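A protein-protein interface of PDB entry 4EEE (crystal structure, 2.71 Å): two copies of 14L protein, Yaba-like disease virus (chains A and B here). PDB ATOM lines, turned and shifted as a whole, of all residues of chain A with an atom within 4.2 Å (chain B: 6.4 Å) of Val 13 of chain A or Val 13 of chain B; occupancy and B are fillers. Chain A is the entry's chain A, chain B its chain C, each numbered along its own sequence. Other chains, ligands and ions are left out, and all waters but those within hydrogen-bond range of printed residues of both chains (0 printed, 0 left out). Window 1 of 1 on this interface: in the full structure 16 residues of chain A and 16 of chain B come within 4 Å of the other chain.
Ile 11 of chain A touches Val 15 of chain B, and with the chains exchanged Val 15 of chain A touches Ile 11 of chain B.
His 12 of chain A touches its own counterpart, His 12 of chain B.
His 12 of chain A touches Pro 14 of chain B, and with the chains exchanged Pro 14 of chain A touches His 12 of chain B.
Val 13 of chain A touches Val 15 of chain B, and with the chains exchanged Val 15 of chain A touches Val 13 of chain B.
O of Ile 11 of chain A is in hydrogen-bond range of N of Val 15 of chain B, at 3.2 Å.
A ring nitrogen (NE2) of His 12 of chain A is in hydrogen-bond range of the backbone carbonyl oxygen (O) of Val 22 of chain B (2.9 Å).
The backbone carbonyl oxygen (O) of Val 13 of chain A lies within hydrogen-bond range of the backbone NH (N) of Val 13 of chain B, 2.6 Å away.
The backbone NH of Val 15 of chain A is in hydrogen-bond range of the backbone carbonyl oxygen of Ile 11 of chain B.
Val 13 of chain A touches just these residues of chain B: Ile 11, His 12, Val 13 and Val 15.
Of chain A, only Ile 11, His 12, Val 13 and Val 15 come within 4 Å of Val 13 of chain B.
Of the printed residues of chain A, Val 22 of chain B touches His 12 (2.9 Å).
Printed residues of chain A within 4 Å of His 12 of chain B: His 12 (3.5 Å), Val 13 (3.0 Å) and Pro 14 (3.3 Å).
Of the printed residues of chain B, Pro 14 of chain A touches Ile 11 and His 12.
Printed residues of chain B within 4 Å of Val 15 of chain A: Ile 11 and Val 13.
Trp 112 of chain B touches none of the printed residues of chain A.
Ile 111 of chain B touches none of the printed residues of chain A.
The nearest residue of chain B that does not touch Val 13 of chain A is Pro 14 of chain B (4.9 Å).
The nearest printed residue of chain A that does not touch Val 13 of chain B is Pro 14 of chain A (4.8 Å).
Printed residues of chain B that touch a printed residue of chain A: Ile 11, His 12, Val 13, Pro 14, Val 15, Val 22 and Glu 24.
Hydrophobic or aromatic side chains of chain B within 4 Å of the printed part of chain A: His 12, Val 13, Pro 14 and Val 15.
Hydrophobic or aromatic side chains of chain A within 4 Å of the printed part of chain B: His 12, Val 13, Pro 14 and Val 15.
Among the printed residues, no Asp or Glu carboxylate lies within 4 Å of a Lys or Arg side-chain nitrogen of the other chain.
The backbone NH of His 12 of chain B is in hydrogen-bond range of the backbone carbonyl oxygen of Glu 24 of chain B (2.8 Å).
The backbone carbonyl oxygen (O) of Pro 14 of chain B sits at hydrogen-bond distance from the indole nitrogen (NE1) of Trp 112 of chain B, 2.9 Å away.
Among the printed residues, merely in contact across the chains: Val 13 of chain A with His 12 of chain B (3.0 Å), His 12 of chain A with Val 13 of chain B (3.2 Å), Pro 14 of chain A with His 12 of chain B (3.3 Å), Pro 14 of chain A with Ile 11 of chain B (3.4 Å), Ile 11 of chain A with Pro 14 of chain B (3.5 Å), His 12 of chain A with His 12 of chain B (3.5 Å), His 12 of chain A with Pro 14 of chain B (3.6 Å), Val 15 of chain A with Val 13 of chain B (3.7 Å), Val 13 of chain A with Ile 11 of chain B (3.7 Å), Ile 11 of chain A with Val 13 of chain B (3.7 Å), Val 13 of chain A with Val 15 of chain B (3.9 Å) and His 12 of chain A with Glu 24 of chain B (3.9 Å).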
ATOM      1  N   ILE A  11      -6.507  14.374  29.401  1.00  0.00           N
ATOM      2  CA  ILE A  11      -7.354  14.193  30.566  1.00  0.00           C
ATOM      3  C   ILE A  11      -8.822  14.102  30.169  1.00  0.00           C
ATOM      4  O   ILE A  11      -9.326  14.931  29.397  1.00  0.00           O
ATOM      5  CB  ILE A  11      -7.217  15.348  31.566  1.00  0.00           C
ATOM      6  CG1 ILE A  11      -5.749  15.579  31.934  1.00  0.00           C
ATOM      7  CG2 ILE A  11      -8.068  15.069  32.806  1.00  0.00           C
ATOM      8  CD1 ILE A  11      -5.508  16.903  32.615  1.00  0.00           C
ATOM      9  N   HIS A  12      -9.507  13.092  30.694  1.00  0.00           N
ATOM     10  CA  HIS A  12     -10.954  13.036  30.572  1.00  0.00           C
ATOM     11  C   HIS A  12     -11.606  13.543  31.854  1.00  0.00           C
ATOM     12  O   HIS A  12     -11.395  12.988  32.933  1.00  0.00           O
ATOM     13  CB  HIS A  12     -11.429  11.627  30.223  1.00  0.00           C
ATOM     14  CG  HIS A  12     -11.419  11.344  28.751  1.00  0.00           C
ATOM     15  ND1 HIS A  12     -10.253  11.187  28.031  1.00  0.00           N
ATOM     16  CD2 HIS A  12     -12.433  11.210  27.865  1.00  0.00           C
ATOM     17  CE1 HIS A  12     -10.551  10.958  26.763  1.00  0.00           C
ATOM     18  NE2 HIS A  12     -11.866  10.967  26.634  1.00  0.00           N
ATOM     19  N   VAL A  13     -12.381  14.615  31.728  1.00  0.00           N
ATOM     20  CA  VAL A  13     -13.108  15.176  32.861  1.00  0.00           C
ATOM     21  C   VAL A  13     -14.601  14.888  32.776  1.00  0.00           C
ATOM     22  O   VAL A  13     -15.158  14.755  31.683  1.00  0.00           O
ATOM     23  CB  VAL A  13     -12.930  16.701  32.976  1.00  0.00           C
ATOM     24  CG1 VAL A  13     -11.496  17.048  33.318  1.00  0.00           C
ATOM     25  CG2 VAL A  13     -13.375  17.398  31.686  1.00  0.00           C
ATOM     26  N   PRO A  14     -15.256  14.791  33.941  1.00  0.00           N
ATOM     27  CA  PRO A  14     -16.718  14.744  34.053  1.00  0.00           C
ATOM     28  C   PRO A  14     -17.312  16.119  33.743  1.00  0.00           C
ATOM     29  O   PRO A  14     -16.738  17.141  34.138  1.00  0.00           O
ATOM     30  CB  PRO A  14     -16.938  14.395  35.526  1.00  0.00           C
ATOM     31  CG  PRO A  14     -15.724  14.947  36.216  1.00  0.00           C
ATOM     32  CD  PRO A  14     -14.599  14.697  35.256  1.00  0.00           C
ATOM     33  N   VAL A  15     -18.437  16.138  33.034  1.00  0.00           N
ATOM     34  CA  VAL A  15     -19.063  17.392  32.620  1.00  0.00           C
ATOM     35  C   VAL A  15     -19.820  18.080  33.766  1.00  0.00           C
ATOM     36  O   VAL A  15     -20.236  19.233  33.639  1.00  0.00           O
ATOM     37  CB  VAL A  15     -20.018  17.176  31.421  1.00  0.00           C
ATOM     38  CG1 VAL A  15     -19.240  16.680  30.210  1.00  0.00           C
ATOM     39  CG2 VAL A  15     -21.127  16.190  31.781  1.00  0.00           C
ATOM     40  N   LEU A  23     -10.851  12.030  37.556  1.00  0.00           N
ATOM     41  CA  LEU A  23     -10.183  12.536  36.353  1.00  0.00           C
ATOM     42  C   LEU A  23      -9.269  11.462  35.766  1.00  0.00           C
ATOM     43  O   LEU A  23      -8.407  10.905  36.460  1.00  0.00           O
ATOM     44  CB  LEU A  23      -9.378  13.798  36.658  1.00  0.00           C
ATOM     45  CG  LEU A  23     -10.102  14.907  37.419  1.00  0.00           C
ATOM     46  CD1 LEU A  23      -9.132  15.992  37.833  1.00  0.00           C
ATOM     47  CD2 LEU A  23     -11.219  15.494  36.586  1.00  0.00           C
ATOM     48  N   ILE B  11     -21.124  12.162  31.814  1.00  0.00           N
ATOM     49  CA  ILE B  11     -20.233  12.057  30.671  1.00  0.00           C
ATOM     50  C   ILE B  11     -18.844  12.567  31.008  1.00  0.00           C
ATOM     51  O   ILE B  11     -18.690  13.657  31.569  1.00  0.00           O
ATOM     52  CB  ILE B  11     -20.740  12.868  29.475  1.00  0.00           C
ATOM     53  CG1 ILE B  11     -22.187  12.490  29.153  1.00  0.00           C
ATOM     54  CG2 ILE B  11     -19.816  12.670  28.268  1.00  0.00           C
ATOM     55  CD1 ILE B  11     -22.863  13.468  28.215  1.00  0.00           C
ATOM     56  N   HIS B  12     -17.835  11.777  30.656  1.00  0.00           N
ATOM     57  CA  HIS B  12     -16.461  12.245  30.732  1.00  0.00           C
ATOM     58  C   HIS B  12     -15.994  12.692  29.349  1.00  0.00           C
ATOM     59  O   HIS B  12     -15.975  11.903  28.397  1.00  0.00           O
ATOM     60  CB  HIS B  12     -15.535  11.177  31.317  1.00  0.00           C
ATOM     61  CG  HIS B  12     -15.473  11.192  32.810  1.00  0.00           C
ATOM     62  ND1 HIS B  12     -16.518  10.768  33.604  1.00  0.00           N
ATOM     63  CD2 HIS B  12     -14.495  11.596  33.660  1.00  0.00           C
ATOM     64  CE1 HIS B  12     -16.187  10.909  34.876  1.00  0.00           C
ATOM     65  NE2 HIS B  12     -14.963  11.407  34.935  1.00  0.00           N
ATOM     66  N   VAL B  13     -15.643  13.971  29.243  1.00  0.00           N
ATOM     67  CA  VAL B  13     -15.108  14.516  27.995  1.00  0.00           C
ATOM     68  C   VAL B  13     -13.603  14.766  28.066  1.00  0.00           C
ATOM     69  O   VAL B  13     -13.055  15.032  29.136  1.00  0.00           O
ATOM     70  CB  VAL B  13     -15.795  15.833  27.602  1.00  0.00           C
ATOM     71  CG1 VAL B  13     -17.266  15.588  27.282  1.00  0.00           C
ATOM     72  CG2 VAL B  13     -15.633  16.868  28.718  1.00  0.00           C
ATOM     73  N   PRO B  14     -12.931  14.679  26.908  1.00  0.00           N
ATOM     74  CA  PRO B  14     -11.536  15.121  26.746  1.00  0.00           C
ATOM     75  C   PRO B  14     -11.455  16.647  26.774  1.00  0.00           C
ATOM     76  O   PRO B  14     -12.330  17.324  26.229  1.00  0.00           O
ATOM     77  CB  PRO B  14     -11.167  14.597  25.353  1.00  0.00           C
ATOM     78  CG  PRO B  14     -12.474  14.528  24.621  1.00  0.00           C
ATOM     79  CD  PRO B  14     -13.486  14.118  25.662  1.00  0.00           C
ATOM     80  N   VAL B  15     -10.423  17.185  27.415  1.00  0.00           N
ATOM     81  CA  VAL B  15     -10.297  18.633  27.558  1.00  0.00           C
ATOM     82  C   VAL B  15      -9.827  19.311  26.267  1.00  0.00           C
ATOM     83  O   VAL B  15      -9.873  20.535  26.144  1.00  0.00           O
ATOM     84  CB  VAL B  15      -9.352  18.999  28.717  1.00  0.00           C
ATOM     85  CG1 VAL B  15      -9.928  18.524  30.040  1.00  0.00           C
ATOM     86  CG2 VAL B  15      -7.970  18.393  28.487  1.00  0.00           C
ATOM     87  N   LYS B  16      -9.374  18.506  25.311  1.00  0.00           N
ATOM     88  CA  LYS B  16      -8.904  19.021  24.024  1.00  0.00           C
ATOM     89  C   LYS B  16      -9.231  18.027  22.924  1.00  0.00           C
ATOM     90  O   LYS B  16      -9.279  16.821  23.164  1.00  0.00           O
ATOM     91  CB  LYS B  16      -7.395  19.270  24.064  1.00  0.00           C
ATOM     92  CG  LYS B  16      -6.582  17.997  23.878  1.00  0.00           C
ATOM     93  CD  LYS B  16      -5.192  18.135  24.490  1.00  0.00           C
ATOM     94  CE  LYS B  16      -4.352  16.875  24.275  1.00  0.00           C
ATOM     95  NZ  LYS B  16      -2.976  17.038  24.843  1.00  0.00           N
ATOM     96  N   VAL B  22     -13.084  10.399  22.192  1.00  0.00           N
ATOM     97  CA  VAL B  22     -13.978   9.476  22.888  1.00  0.00           C
ATOM     98  C   VAL B  22     -14.717  10.145  24.043  1.00  0.00           C
ATOM     99  O   VAL B  22     -14.106  10.824  24.868  1.00  0.00           O
ATOM    100  CB  VAL B  22     -13.227   8.244  23.408  1.00  0.00           C
ATOM    101  CG1 VAL B  22     -14.213   7.231  23.982  1.00  0.00           C
ATOM    102  CG2 VAL B  22     -12.415   7.627  22.291  1.00  0.00           C
ATOM    103  N   LEU B  23     -16.035   9.947  24.086  1.00  0.00           N
ATOM    104  CA  LEU B  23     -16.861  10.415  25.200  1.00  0.00           C
ATOM    105  C   LEU B  23     -17.351   9.223  26.015  1.00  0.00           C
ATOM    106  O   LEU B  23     -17.938   8.276  25.472  1.00  0.00           O
ATOM    107  CB  LEU B  23     -18.057  11.224  24.698  1.00  0.00           C
ATOM    108  CG  LEU B  23     -17.749  12.336  23.706  1.00  0.00           C
ATOM    109  CD1 LEU B  23     -19.044  12.922  23.169  1.00  0.00           C
ATOM    110  CD2 LEU B  23     -16.898  13.411  24.354  1.00  0.00           C
ATOM    111  N   GLU B  24     -17.105   9.265  27.318  1.00  0.00           N
ATOM    112  CA  GLU B  24     -17.522   8.180  28.200  1.00  0.00           C
ATOM    113  C   GLU B  24     -18.812   8.507  28.948  1.00  0.00           C
ATOM    114  O   GLU B  24     -18.811   9.325  29.875  1.00  0.00           O
ATOM    115  CB  GLU B  24     -16.414   7.856  29.206  1.00  0.00           C
ATOM    116  CG  GLU B  24     -15.243   7.090  28.611  1.00  0.00           C
ATOM    117  CD  GLU B  24     -13.970   7.273  29.407  1.00  0.00           C
ATOM    118  OE1 GLU B  24     -13.854   8.296  30.110  1.00  0.00           O
ATOM    119  OE2 GLU B  24     -13.086   6.399  29.336  1.00  0.00           O
ATOM    120  N   VAL B 106     -24.183  17.644  26.031  1.00  0.00           N
ATOM    121  CA  VAL B 106     -22.930  18.385  25.929  1.00  0.00           C
ATOM    122  C   VAL B 106     -22.684  18.900  24.517  1.00  0.00           C
ATOM    123  O   VAL B 106     -23.066  18.264  23.539  1.00  0.00           O
ATOM    124  CB  VAL B 106     -21.739  17.514  26.363  1.00  0.00           C
ATOM    125  N   LEU B 108     -19.251  19.893  22.501  1.00  0.00           N
ATOM    126  CA  LEU B 108     -17.785  19.888  22.567  1.00  0.00           C
ATOM    127  C   LEU B 108     -17.135  21.256  22.340  1.00  0.00           C
ATOM    128  O   LEU B 108     -16.239  21.646  23.090  1.00  0.00           O
ATOM    129  CB  LEU B 108     -17.199  18.853  21.601  1.00  0.00           C
ATOM    130  CG  LEU B 108     -17.628  17.414  21.901  1.00  0.00           C
ATOM    131  CD1 LEU B 108     -17.395  16.479  20.719  1.00  0.00           C
ATOM    132  CD2 LEU B 108     -16.940  16.878  23.158  1.00  0.00           C
ATOM    133  N   ILE B 111     -16.964  23.496  25.292  1.00  0.00           N
ATOM    134  CA  ILE B 111     -16.029  23.056  26.317  1.00  0.00           C
ATOM    135  C   ILE B 111     -14.595  23.365  25.923  1.00  0.00           C
ATOM    136  O   ILE B 111     -13.852  23.988  26.681  1.00  0.00           O
ATOM    137  CB  ILE B 111     -16.179  21.548  26.586  1.00  0.00           C
ATOM    138  CG1 ILE B 111     -17.511  21.278  27.297  1.00  0.00           C
ATOM    139  CG2 ILE B 111     -15.005  21.026  27.411  1.00  0.00           C
ATOM    140  CD1 ILE B 111     -17.673  19.868  27.800  1.00  0.00           C
ATOM    141  N   TRP B 112     -14.211  22.933  24.726  1.00  0.00           N
ATOM    142  CA  TRP B 112     -12.871  23.201  24.222  1.00  0.00           C
ATOM    143  C   TRP B 112     -12.583  24.705  24.160  1.00  0.00           C
ATOM    144  O   TRP B 112     -11.433  25.119  24.043  1.00  0.00           O
ATOM    145  CB  TRP B 112     -12.659  22.506  22.872  1.00  0.00           C
ATOM    146  CG  TRP B 112     -12.674  21.003  22.976  1.00  0.00           C
ATOM    147  CD1 TRP B 112     -12.308  20.254  24.054  1.00  0.00           C
ATOM    148  CD2 TRP B 112     -13.093  20.073  21.965  1.00  0.00           C
ATOM    149  NE1 TRP B 112     -12.469  18.915  23.777  1.00  0.00           N
ATOM    150  CE2 TRP B 112     -12.952  18.777  22.502  1.00  0.00           C
ATOM    151  CE3 TRP B 112     -13.577  20.214  20.663  1.00  0.00           C
ATOM    152  CZ2 TRP B 112     -13.274  17.628  21.778  1.00  0.00           C
ATOM    153  CZ3 TRP B 112     -13.896  19.074  19.945  1.00  0.00           C
ATOM    154  CH2 TRP B 112     -13.745  17.797  20.504  1.00  0.00           C
